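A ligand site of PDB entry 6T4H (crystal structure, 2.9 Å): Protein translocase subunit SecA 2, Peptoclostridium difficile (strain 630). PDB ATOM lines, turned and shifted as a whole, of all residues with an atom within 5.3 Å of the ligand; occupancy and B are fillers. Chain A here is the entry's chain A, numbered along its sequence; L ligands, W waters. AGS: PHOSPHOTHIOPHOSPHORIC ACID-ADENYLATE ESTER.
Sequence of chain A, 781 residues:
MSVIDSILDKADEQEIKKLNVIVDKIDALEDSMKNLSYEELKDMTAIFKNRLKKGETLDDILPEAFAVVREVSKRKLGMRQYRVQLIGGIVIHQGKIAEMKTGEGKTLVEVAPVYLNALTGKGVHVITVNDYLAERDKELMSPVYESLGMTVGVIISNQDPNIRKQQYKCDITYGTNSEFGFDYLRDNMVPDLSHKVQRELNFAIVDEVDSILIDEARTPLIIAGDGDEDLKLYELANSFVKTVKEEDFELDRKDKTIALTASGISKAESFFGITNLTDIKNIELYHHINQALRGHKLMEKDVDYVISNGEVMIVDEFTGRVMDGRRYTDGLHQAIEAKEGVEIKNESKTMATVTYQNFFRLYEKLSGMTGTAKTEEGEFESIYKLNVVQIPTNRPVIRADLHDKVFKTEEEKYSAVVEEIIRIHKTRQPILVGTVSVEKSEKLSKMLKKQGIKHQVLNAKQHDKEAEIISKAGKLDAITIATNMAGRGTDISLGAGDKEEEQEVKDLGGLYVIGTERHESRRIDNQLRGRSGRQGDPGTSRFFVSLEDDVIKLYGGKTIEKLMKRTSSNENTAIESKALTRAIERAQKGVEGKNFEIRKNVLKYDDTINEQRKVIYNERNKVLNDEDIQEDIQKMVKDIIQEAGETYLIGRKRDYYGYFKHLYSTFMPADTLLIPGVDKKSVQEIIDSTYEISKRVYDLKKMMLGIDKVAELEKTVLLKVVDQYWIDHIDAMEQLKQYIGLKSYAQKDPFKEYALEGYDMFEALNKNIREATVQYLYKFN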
ATOM      1  N   MET A  79      -8.331 -18.178  19.772  1.00  0.00           N
ATOM      2  CA  MET A  79      -7.318 -17.175  19.609  1.00  0.00           C
ATOM      3  C   MET A  79      -7.834 -15.782  19.396  1.00  0.00           C
ATOM      4  O   MET A  79      -7.879 -15.307  18.267  1.00  0.00           O
ATOM      5  CB  MET A  79      -6.337 -17.529  18.460  1.00  0.00           C
ATOM      6  CG  MET A  79      -5.169 -18.452  18.827  1.00  0.00           C
ATOM      7  SD  MET A  79      -5.340 -20.221  18.365  1.00  0.00           S
ATOM      8  CE  MET A  79      -4.052 -20.371  17.103  1.00  0.00           C
ATOM      9  N   ARG A  80      -8.241 -15.129  20.452  1.00  0.00           N
ATOM     10  CA  ARG A  80      -8.724 -13.790  20.271  1.00  0.00           C
ATOM     11  C   ARG A  80      -7.427 -13.040  19.811  1.00  0.00           C
ATOM     12  O   ARG A  80      -6.322 -13.601  19.965  1.00  0.00           O
ATOM     13  CB  ARG A  80      -9.319 -13.300  21.581  1.00  0.00           C
ATOM     14  CG  ARG A  80     -10.043 -11.936  21.565  1.00  0.00           C
ATOM     15  CD  ARG A  80      -9.230 -10.748  22.138  1.00  0.00           C
ATOM     16  NE  ARG A  80     -10.105  -9.692  22.680  1.00  0.00           N
ATOM     17  CZ  ARG A  80      -9.652  -8.471  22.952  1.00  0.00           C
ATOM     18  NH1 ARG A  80     -10.463  -7.544  23.445  1.00  0.00           N
ATOM     19  NH2 ARG A  80      -8.384  -8.167  22.742  1.00  0.00           N
ATOM     20  N   GLN A  81      -7.500 -11.835  19.285  1.00  0.00           N
ATOM     21  CA  GLN A  81      -6.238 -11.239  18.871  1.00  0.00           C
ATOM     22  C   GLN A  81      -5.702 -10.160  19.713  1.00  0.00           C
ATOM     23  O   GLN A  81      -6.484  -9.316  20.169  1.00  0.00           O
ATOM     24  CB  GLN A  81      -6.371 -10.738  17.409  1.00  0.00           C
ATOM     25  CG  GLN A  81      -6.271 -11.806  16.289  1.00  0.00           C
ATOM     26  CD  GLN A  81      -7.578 -12.400  15.753  1.00  0.00           C
ATOM     27  OE1 GLN A  81      -7.570 -13.140  14.759  1.00  0.00           O
ATOM     28  NE2 GLN A  81      -8.726 -12.092  16.382  1.00  0.00           N
ATOM     29  N   TYR A  82      -4.372 -10.150  19.948  1.00  0.00           N
ATOM     30  CA  TYR A  82      -3.816  -9.088  20.779  1.00  0.00           C
ATOM     31  C   TYR A  82      -3.278  -7.996  19.923  1.00  0.00           C
ATOM     32  O   TYR A  82      -2.771  -8.290  18.837  1.00  0.00           O
ATOM     33  CB  TYR A  82      -2.673  -9.514  21.699  1.00  0.00           C
ATOM     34  CG  TYR A  82      -2.590 -10.973  22.059  1.00  0.00           C
ATOM     35  CD1 TYR A  82      -1.615 -11.775  21.503  1.00  0.00           C
ATOM     36  CD2 TYR A  82      -3.423 -11.523  23.020  1.00  0.00           C
ATOM     37  CE1 TYR A  82      -1.474 -13.103  21.890  1.00  0.00           C
ATOM     38  CE2 TYR A  82      -3.287 -12.844  23.423  1.00  0.00           C
ATOM     39  CZ  TYR A  82      -2.308 -13.633  22.856  1.00  0.00           C
ATOM     40  OH  TYR A  82      -2.158 -14.940  23.243  1.00  0.00           O
ATOM     41  N   GLN A  85      -0.637  -8.491  17.648  1.00  0.00           N
ATOM     42  CA  GLN A  85      -0.979  -9.358  16.556  1.00  0.00           C
ATOM     43  C   GLN A  85      -1.839  -8.618  15.528  1.00  0.00           C
ATOM     44  O   GLN A  85      -2.025  -9.105  14.417  1.00  0.00           O
ATOM     45  CB  GLN A  85      -1.702 -10.612  17.070  1.00  0.00           C
ATOM     46  CG  GLN A  85      -0.798 -11.677  17.672  1.00  0.00           C
ATOM     47  CD  GLN A  85      -1.658 -12.846  18.017  1.00  0.00           C
ATOM     48  OE1 GLN A  85      -2.603 -12.728  18.804  1.00  0.00           O
ATOM     49  NE2 GLN A  85      -1.301 -14.050  17.492  1.00  0.00           N
ATOM     50  N   MET A 100       8.172  -9.982  14.185  1.00  0.00           N
ATOM     51  CA  MET A 100       7.634 -10.460  15.459  1.00  0.00           C
ATOM     52  C   MET A 100       8.584 -11.548  15.928  1.00  0.00           C
ATOM     53  O   MET A 100       9.154 -12.228  15.073  1.00  0.00           O
ATOM     54  CB  MET A 100       6.245 -11.041  15.258  1.00  0.00           C
ATOM     55  CG  MET A 100       5.290 -10.032  14.724  1.00  0.00           C
ATOM     56  SD  MET A 100       3.611 -10.539  15.004  1.00  0.00           S
ATOM     57  CE  MET A 100       2.784  -9.154  14.408  1.00  0.00           C
ATOM     58  N   LYS A 101       8.774 -11.751  17.236  1.00  0.00           N
ATOM     59  CA  LYS A 101       9.722 -12.815  17.577  1.00  0.00           C
ATOM     60  C   LYS A 101       9.133 -14.227  17.676  1.00  0.00           C
ATOM     61  O   LYS A 101       7.908 -14.332  17.766  1.00  0.00           O
ATOM     62  CB  LYS A 101      10.568 -12.353  18.770  1.00  0.00           C
ATOM     63  CG  LYS A 101      10.875 -10.824  18.714  1.00  0.00           C
ATOM     64  CD  LYS A 101      12.305 -10.445  18.158  1.00  0.00           C
ATOM     65  CE  LYS A 101      12.651  -8.959  18.288  1.00  0.00           C
ATOM     66  NZ  LYS A 101      13.985  -8.521  17.707  1.00  0.00           N
ATOM     67  N   THR A 102       9.976 -15.310  17.652  1.00  0.00           N
ATOM     68  CA  THR A 102       9.370 -16.639  17.738  1.00  0.00           C
ATOM     69  C   THR A 102       8.327 -16.779  18.780  1.00  0.00           C
ATOM     70  O   THR A 102       8.412 -16.188  19.842  1.00  0.00           O
ATOM     71  CB  THR A 102      10.370 -17.753  17.872  1.00  0.00           C
ATOM     72  OG1 THR A 102      11.460 -17.496  16.982  1.00  0.00           O
ATOM     73  CG2 THR A 102       9.741 -19.185  17.631  1.00  0.00           C
ATOM     74  N   GLY A 103       7.307 -17.557  18.452  1.00  0.00           N
ATOM     75  CA  GLY A 103       6.197 -17.797  19.353  1.00  0.00           C
ATOM     76  C   GLY A 103       5.260 -16.620  19.445  1.00  0.00           C
ATOM     77  O   GLY A 103       4.279 -16.708  20.181  1.00  0.00           O
ATOM     78  N   GLU A 104       5.529 -15.506  18.710  1.00  0.00           N
ATOM     79  CA  GLU A 104       4.593 -14.387  18.836  1.00  0.00           C
ATOM     80  C   GLU A 104       3.237 -14.581  18.164  1.00  0.00           C
ATOM     81  O   GLU A 104       2.390 -13.673  18.250  1.00  0.00           O
ATOM     82  CB  GLU A 104       5.202 -13.076  18.359  1.00  0.00           C
ATOM     83  CG  GLU A 104       5.936 -12.281  19.423  1.00  0.00           C
ATOM     84  CD  GLU A 104       5.166 -11.073  19.953  1.00  0.00           C
ATOM     85  OE1 GLU A 104       5.207 -10.012  19.310  1.00  0.00           O
ATOM     86  OE2 GLU A 104       4.556 -11.214  21.037  1.00  0.00           O
ATOM     87  N   GLY A 105       3.023 -15.738  17.466  1.00  0.00           N
ATOM     88  CA  GLY A 105       1.739 -15.964  16.823  1.00  0.00           C
ATOM     89  C   GLY A 105       1.566 -15.501  15.384  1.00  0.00           C
ATOM     90  O   GLY A 105       0.454 -15.155  14.956  1.00  0.00           O
ATOM     91  N   LYS A 106       2.664 -15.485  14.640  1.00  0.00           N
ATOM     92  CA  LYS A 106       2.629 -15.064  13.255  1.00  0.00           C
ATOM     93  C   LYS A 106       1.551 -15.809  12.406  1.00  0.00           C
ATOM     94  O   LYS A 106       0.834 -15.141  11.646  1.00  0.00           O
ATOM     95  CB  LYS A 106       4.032 -15.225  12.635  1.00  0.00           C
ATOM     96  CG  LYS A 106       4.961 -14.074  12.898  1.00  0.00           C
ATOM     97  CD  LYS A 106       6.359 -14.664  12.985  1.00  0.00           C
ATOM     98  CE  LYS A 106       7.492 -13.657  13.057  1.00  0.00           C
ATOM     99  N   THR A 107       1.436 -17.156  12.538  1.00  0.00           N
ATOM    100  CA  THR A 107       0.447 -17.891  11.773  1.00  0.00           C
ATOM    101  C   THR A 107      -0.839 -17.141  11.905  1.00  0.00           C
ATOM    102  O   THR A 107      -1.495 -16.914  10.905  1.00  0.00           O
ATOM    103  CB  THR A 107       0.244 -19.351  12.258  1.00  0.00           C
ATOM    104  OG1 THR A 107       1.432 -20.088  12.027  1.00  0.00           O
ATOM    105  CG2 THR A 107      -0.989 -19.998  11.647  1.00  0.00           C
ATOM    106  N   LEU A 108      -1.214 -16.734  13.084  1.00  0.00           N
ATOM    107  CA  LEU A 108      -2.476 -16.008  13.136  1.00  0.00           C
ATOM    108  C   LEU A 108      -2.319 -14.535  12.728  1.00  0.00           C
ATOM    109  O   LEU A 108      -3.316 -13.936  12.346  1.00  0.00           O
ATOM    110  CB  LEU A 108      -3.166 -16.074  14.499  1.00  0.00           C
ATOM    111  CG  LEU A 108      -4.639 -15.766  14.477  1.00  0.00           C
ATOM    112  CD1 LEU A 108      -5.352 -17.132  14.505  1.00  0.00           C
ATOM    113  CD2 LEU A 108      -5.048 -14.777  15.642  1.00  0.00           C
ATOM    114  N   ARG A 136      -0.586 -27.529   7.319  1.00  0.00           N
ATOM    115  CA  ARG A 136      -0.954 -27.353   8.700  1.00  0.00           C
ATOM    116  C   ARG A 136      -1.500 -25.965   8.886  1.00  0.00           C
ATOM    117  O   ARG A 136      -2.548 -25.799   9.494  1.00  0.00           O
ATOM    118  CB  ARG A 136       0.337 -27.501   9.600  1.00  0.00           C
ATOM    119  CG  ARG A 136       0.331 -26.797  11.007  1.00  0.00           C
ATOM    120  CD  ARG A 136       1.685 -26.335  11.557  1.00  0.00           C
ATOM    121  NE  ARG A 136       1.881 -24.875  11.396  1.00  0.00           N
ATOM    122  CZ  ARG A 136       2.597 -24.128  12.217  1.00  0.00           C
ATOM    123  NH1 ARG A 136       3.199 -24.684  13.265  1.00  0.00           N
ATOM    124  NH2 ARG A 136       2.718 -22.817  12.009  1.00  0.00           N
ATOM    125  N   ASP A 137      -0.794 -24.963   8.350  1.00  0.00           N
ATOM    126  CA  ASP A 137      -1.246 -23.577   8.472  1.00  0.00           C
ATOM    127  C   ASP A 137      -2.632 -23.396   7.906  1.00  0.00           C
ATOM    128  O   ASP A 137      -3.460 -22.730   8.531  1.00  0.00           O
ATOM    129  CB  ASP A 137      -0.234 -22.615   7.818  1.00  0.00           C
ATOM    130  CG  ASP A 137       0.837 -22.125   8.773  1.00  0.00           C
ATOM    131  OD1 ASP A 137       0.851 -22.568   9.943  1.00  0.00           O
ATOM    132  OD2 ASP A 137       1.675 -21.307   8.337  1.00  0.00           O
ATOM    133  N   ASP A 207       5.832 -16.080   4.933  1.00  0.00           N
ATOM    134  CA  ASP A 207       6.113 -16.475   6.314  1.00  0.00           C
ATOM    135  C   ASP A 207       7.603 -16.741   6.445  1.00  0.00           C
ATOM    136  O   ASP A 207       8.165 -17.470   5.630  1.00  0.00           O
ATOM    137  CB  ASP A 207       5.320 -17.746   6.679  1.00  0.00           C
ATOM    138  CG  ASP A 207       5.263 -18.069   8.164  1.00  0.00           C
ATOM    139  OD1 ASP A 207       4.594 -19.057   8.531  1.00  0.00           O
ATOM    140  OD2 ASP A 207       5.882 -17.333   8.959  1.00  0.00           O
ATOM    141  N   GLU A 208       8.264 -16.124   7.457  1.00  0.00           N
ATOM    142  CA  GLU A 208       9.694 -16.324   7.647  1.00  0.00           C
ATOM    143  C   GLU A 208      10.403 -15.777   6.441  1.00  0.00           C
ATOM    144  O   GLU A 208      11.273 -16.416   5.847  1.00  0.00           O
ATOM    145  CB  GLU A 208      10.009 -17.819   7.844  1.00  0.00           C
ATOM    146  CG  GLU A 208       9.782 -18.313   9.255  1.00  0.00           C
ATOM    147  CD  GLU A 208      10.311 -19.717   9.472  1.00  0.00           C
ATOM    148  OE1 GLU A 208       9.544 -20.685   9.267  1.00  0.00           O
ATOM    149  OE2 GLU A 208      11.502 -19.849   9.822  1.00  0.00           O
ATOM    150  N   MET A 369       6.434 -11.758   7.092  1.00  0.00           N
ATOM    151  CA  MET A 369       6.725 -11.620   8.521  1.00  0.00           C
ATOM    152  C   MET A 369       7.955 -12.413   8.870  1.00  0.00           C
ATOM    153  O   MET A 369       8.319 -13.334   8.144  1.00  0.00           O
ATOM    154  CB  MET A 369       5.609 -12.188   9.372  1.00  0.00           C
ATOM    155  CG  MET A 369       4.310 -11.747   8.975  1.00  0.00           C
ATOM    156  SD  MET A 369       3.079 -13.048   9.406  1.00  0.00           S
ATOM    157  CE  MET A 369       3.971 -14.660   8.846  1.00  0.00           C
ATOM    158  N   ARG A 488      10.324 -26.538  12.955  1.00  0.00           N
ATOM    159  CA  ARG A 488      10.363 -25.080  12.917  1.00  0.00           C
ATOM    160  C   ARG A 488       9.180 -24.310  13.460  1.00  0.00           C
ATOM    161  O   ARG A 488       9.273 -23.722  14.540  1.00  0.00           O
ATOM    162  CB  ARG A 488      10.683 -24.607  11.484  1.00  0.00           C
ATOM    163  CG  ARG A 488      11.894 -23.689  11.398  1.00  0.00           C
ATOM    164  CD  ARG A 488      12.032 -23.008  10.045  1.00  0.00           C
ATOM    165  NE  ARG A 488      12.989 -23.657   9.157  1.00  0.00           N
ATOM    166  CZ  ARG A 488      13.910 -23.000   8.471  1.00  0.00           C
ATOM    167  NH1 ARG A 488      14.744 -23.655   7.681  1.00  0.00           N
ATOM    168  NH2 ARG A 488      14.006 -21.678   8.575  1.00  0.00           N
ATOM    169  N   GLY A 489       8.060 -24.283  12.720  1.00  0.00           N
ATOM    170  CA  GLY A 489       6.893 -23.547  13.184  1.00  0.00           C
ATOM    171  C   GLY A 489       6.203 -24.077  14.417  1.00  0.00           C
ATOM    172  O   GLY A 489       5.227 -23.471  14.876  1.00  0.00           O
ATOM    173  N   ASP A 491       5.522 -24.943  18.418  1.00  0.00           N
ATOM    174  CA  ASP A 491       5.773 -24.171  19.601  1.00  0.00           C
ATOM    175  C   ASP A 491       6.350 -24.961  20.745  1.00  0.00           C
ATOM    176  O   ASP A 491       6.122 -26.169  20.861  1.00  0.00           O
ATOM    177  CB  ASP A 491       4.488 -23.467  20.035  1.00  0.00           C
ATOM    178  CG  ASP A 491       4.693 -22.263  20.910  1.00  0.00           C
ATOM    179  OD1 ASP A 491       5.826 -21.726  20.929  1.00  0.00           O
ATOM    180  OD2 ASP A 491       3.724 -21.817  21.517  1.00  0.00           O
HETATM  181  PG  AGS L   1       5.782 -19.008  12.742  1.00  0.00           P
HETATM  182  S1G AGS L   1       4.048 -19.523  12.129  1.00  0.00           S
HETATM  183  O2G AGS L   1       6.418 -17.910  11.888  1.00  0.00           O
HETATM  184  O3G AGS L   1       6.653 -20.186  13.175  1.00  0.00           O
HETATM  185  PB  AGS L   1       5.579 -17.807  15.396  1.00  0.00           P
HETATM  186  O1B AGS L   1       6.625 -18.792  15.894  1.00  0.00           O
HETATM  187  O2B AGS L   1       5.896 -16.320  15.351  1.00  0.00           O
HETATM  188  O3B AGS L   1       5.030 -18.363  13.991  1.00  0.00           O
HETATM  189  PA  AGS L   1       3.249 -19.164  16.079  1.00  0.00           P
HETATM  190  O1A AGS L   1       2.089 -18.716  15.203  1.00  0.00           O
HETATM  191  O2A AGS L   1       4.009 -20.372  15.553  1.00  0.00           O
HETATM  192  O3A AGS L   1       4.292 -17.984  16.285  1.00  0.00           O
HETATM  193  O5' AGS L   1       2.698 -19.497  17.504  1.00  0.00           O
HETATM  194  C5' AGS L   1       1.706 -20.423  17.482  1.00  0.00           C
HETATM  195  C4' AGS L   1       1.267 -20.793  18.874  1.00  0.00           C
HETATM  196  O4' AGS L   1       0.851 -19.594  19.568  1.00  0.00           O
HETATM  197  C3' AGS L   1       0.064 -21.731  18.788  1.00  0.00           C
HETATM  198  O3' AGS L   1       0.015 -22.648  19.854  1.00  0.00           O
HETATM  199  C2' AGS L   1      -1.091 -20.772  18.885  1.00  0.00           C
HETATM  200  O2' AGS L   1      -2.161 -21.439  19.524  1.00  0.00           O
HETATM  201  C1' AGS L   1      -0.534 -19.701  19.827  1.00  0.00           C
HETATM  202  N9  AGS L   1      -1.127 -18.401  19.710  1.00  0.00           N
HETATM  203  C8  AGS L   1      -0.812 -17.402  18.838  1.00  0.00           C
HETATM  204  N7  AGS L   1      -1.569 -16.283  19.029  1.00  0.00           N
HETATM  205  C5  AGS L   1      -2.367 -16.616  20.043  1.00  0.00           C
HETATM  206  C6  AGS L   1      -3.328 -15.876  20.716  1.00  0.00           C
HETATM  207  N6  AGS L   1      -3.547 -14.604  20.386  1.00  0.00           N
HETATM  208  N1  AGS L   1      -4.045 -16.445  21.712  1.00  0.00           N
HETATM  209  C2  AGS L   1      -3.780 -17.719  22.021  1.00  0.00           C
HETATM  210  N3  AGS L   1      -2.854 -18.498  21.434  1.00  0.00           N
HETATM  211  C4  AGS L   1      -2.131 -17.893  20.464  1.00  0.00           C
HETATM  212  O   HOH W   1       3.111 -23.126  16.500  1.00  0.00           O
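The backbone carbonyl oxygen (O) of Gly 105 lies within hydrogen-bond range of the side-chain amide nitrogen (NE2) of Gln 85 (3.3 Å). The side-chain amide oxygen (OE1) of Gln 85 sits close to the backbone NH (N) of Tyr 82. The side-chain hydroxyl (OG1) of Thr 107 sits at hydrogen-bond distance from the guanidinium group (NH2) of Arg 136 (3.0 Å). OD1 of Asp 137 is in hydrogen-bond range of OG1 of Thr 107 (3.3 Å). O of Gly 489 sits at hydrogen-bond distance from NH1 of Arg 136, at 2.9 Å. NH2 of Arg 136 is in salt-bridge range of OD1 of Asp 137 (2.8 Å).
Water W1 bridges the backbone carbonyl oxygen (O) of Gly 489 (2.7 Å) and an oxygen (O2A) of the ligand (3.0 Å).
The backbone carbonyl oxygen (O) of Gly 489 sits close to an oxygen (O2A) of the ligand. Lys 101 touches the ligand (O to O2B, 3.7 Å). Thr 102 touches the ligand. Asp 491 touches the ligand (OD2 to C4', 3.8 Å). Within 4 Å of the ligand: Met 79, Arg 80, Tyr 82, Gln 85, Lys 101, Thr 102, Gly 103, Glu 104, Gly 105, Lys 106, Thr 107, Arg 136, Asp 207, Gly 489 and Asp 491.
The side-chain amide oxygen (OE1) of Gln 85 is in hydrogen-bond range of a nitrogen (N6) of the ligand (2.6 Å). N of Thr 107 sits at hydrogen-bond distance from O1A of the ligand. The side-chain hydroxyl of Thr 107 sits close to a sulfur (S1G) of the ligand (2.7 Å). O3A of the ligand lies within hydrogen-bond range of N of Gly 105 (2.8 Å). The side-chain hydroxyl of Tyr 82 is in hydrogen-bond range of a nitrogen (N1) of the ligand, 2.9 Å away. The backbone NH (N) of Gly 103 lies within hydrogen-bond range of an oxygen (O1B) of the ligand, 2.9 Å away. An oxygen (O1A) of the ligand sits at hydrogen-bond distance from the backbone NH (N) of Lys 106, at 3.3 Å. O of Arg 80 is in hydrogen-bond range of N6 of the ligand (3.0 Å). The side-chain carboxylate of Asp 207 sits at hydrogen-bond distance from an oxygen (O2G) of the ligand (3.0 Å). O2' of the ligand lies close to SD of Met 79, 3.6 Å away. The backbone NH of Glu 104 sits at hydrogen-bond distance from an oxygen (O2B) of the ligand (3.5 Å). S1G of the ligand lies close to NH2 of Arg 136.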
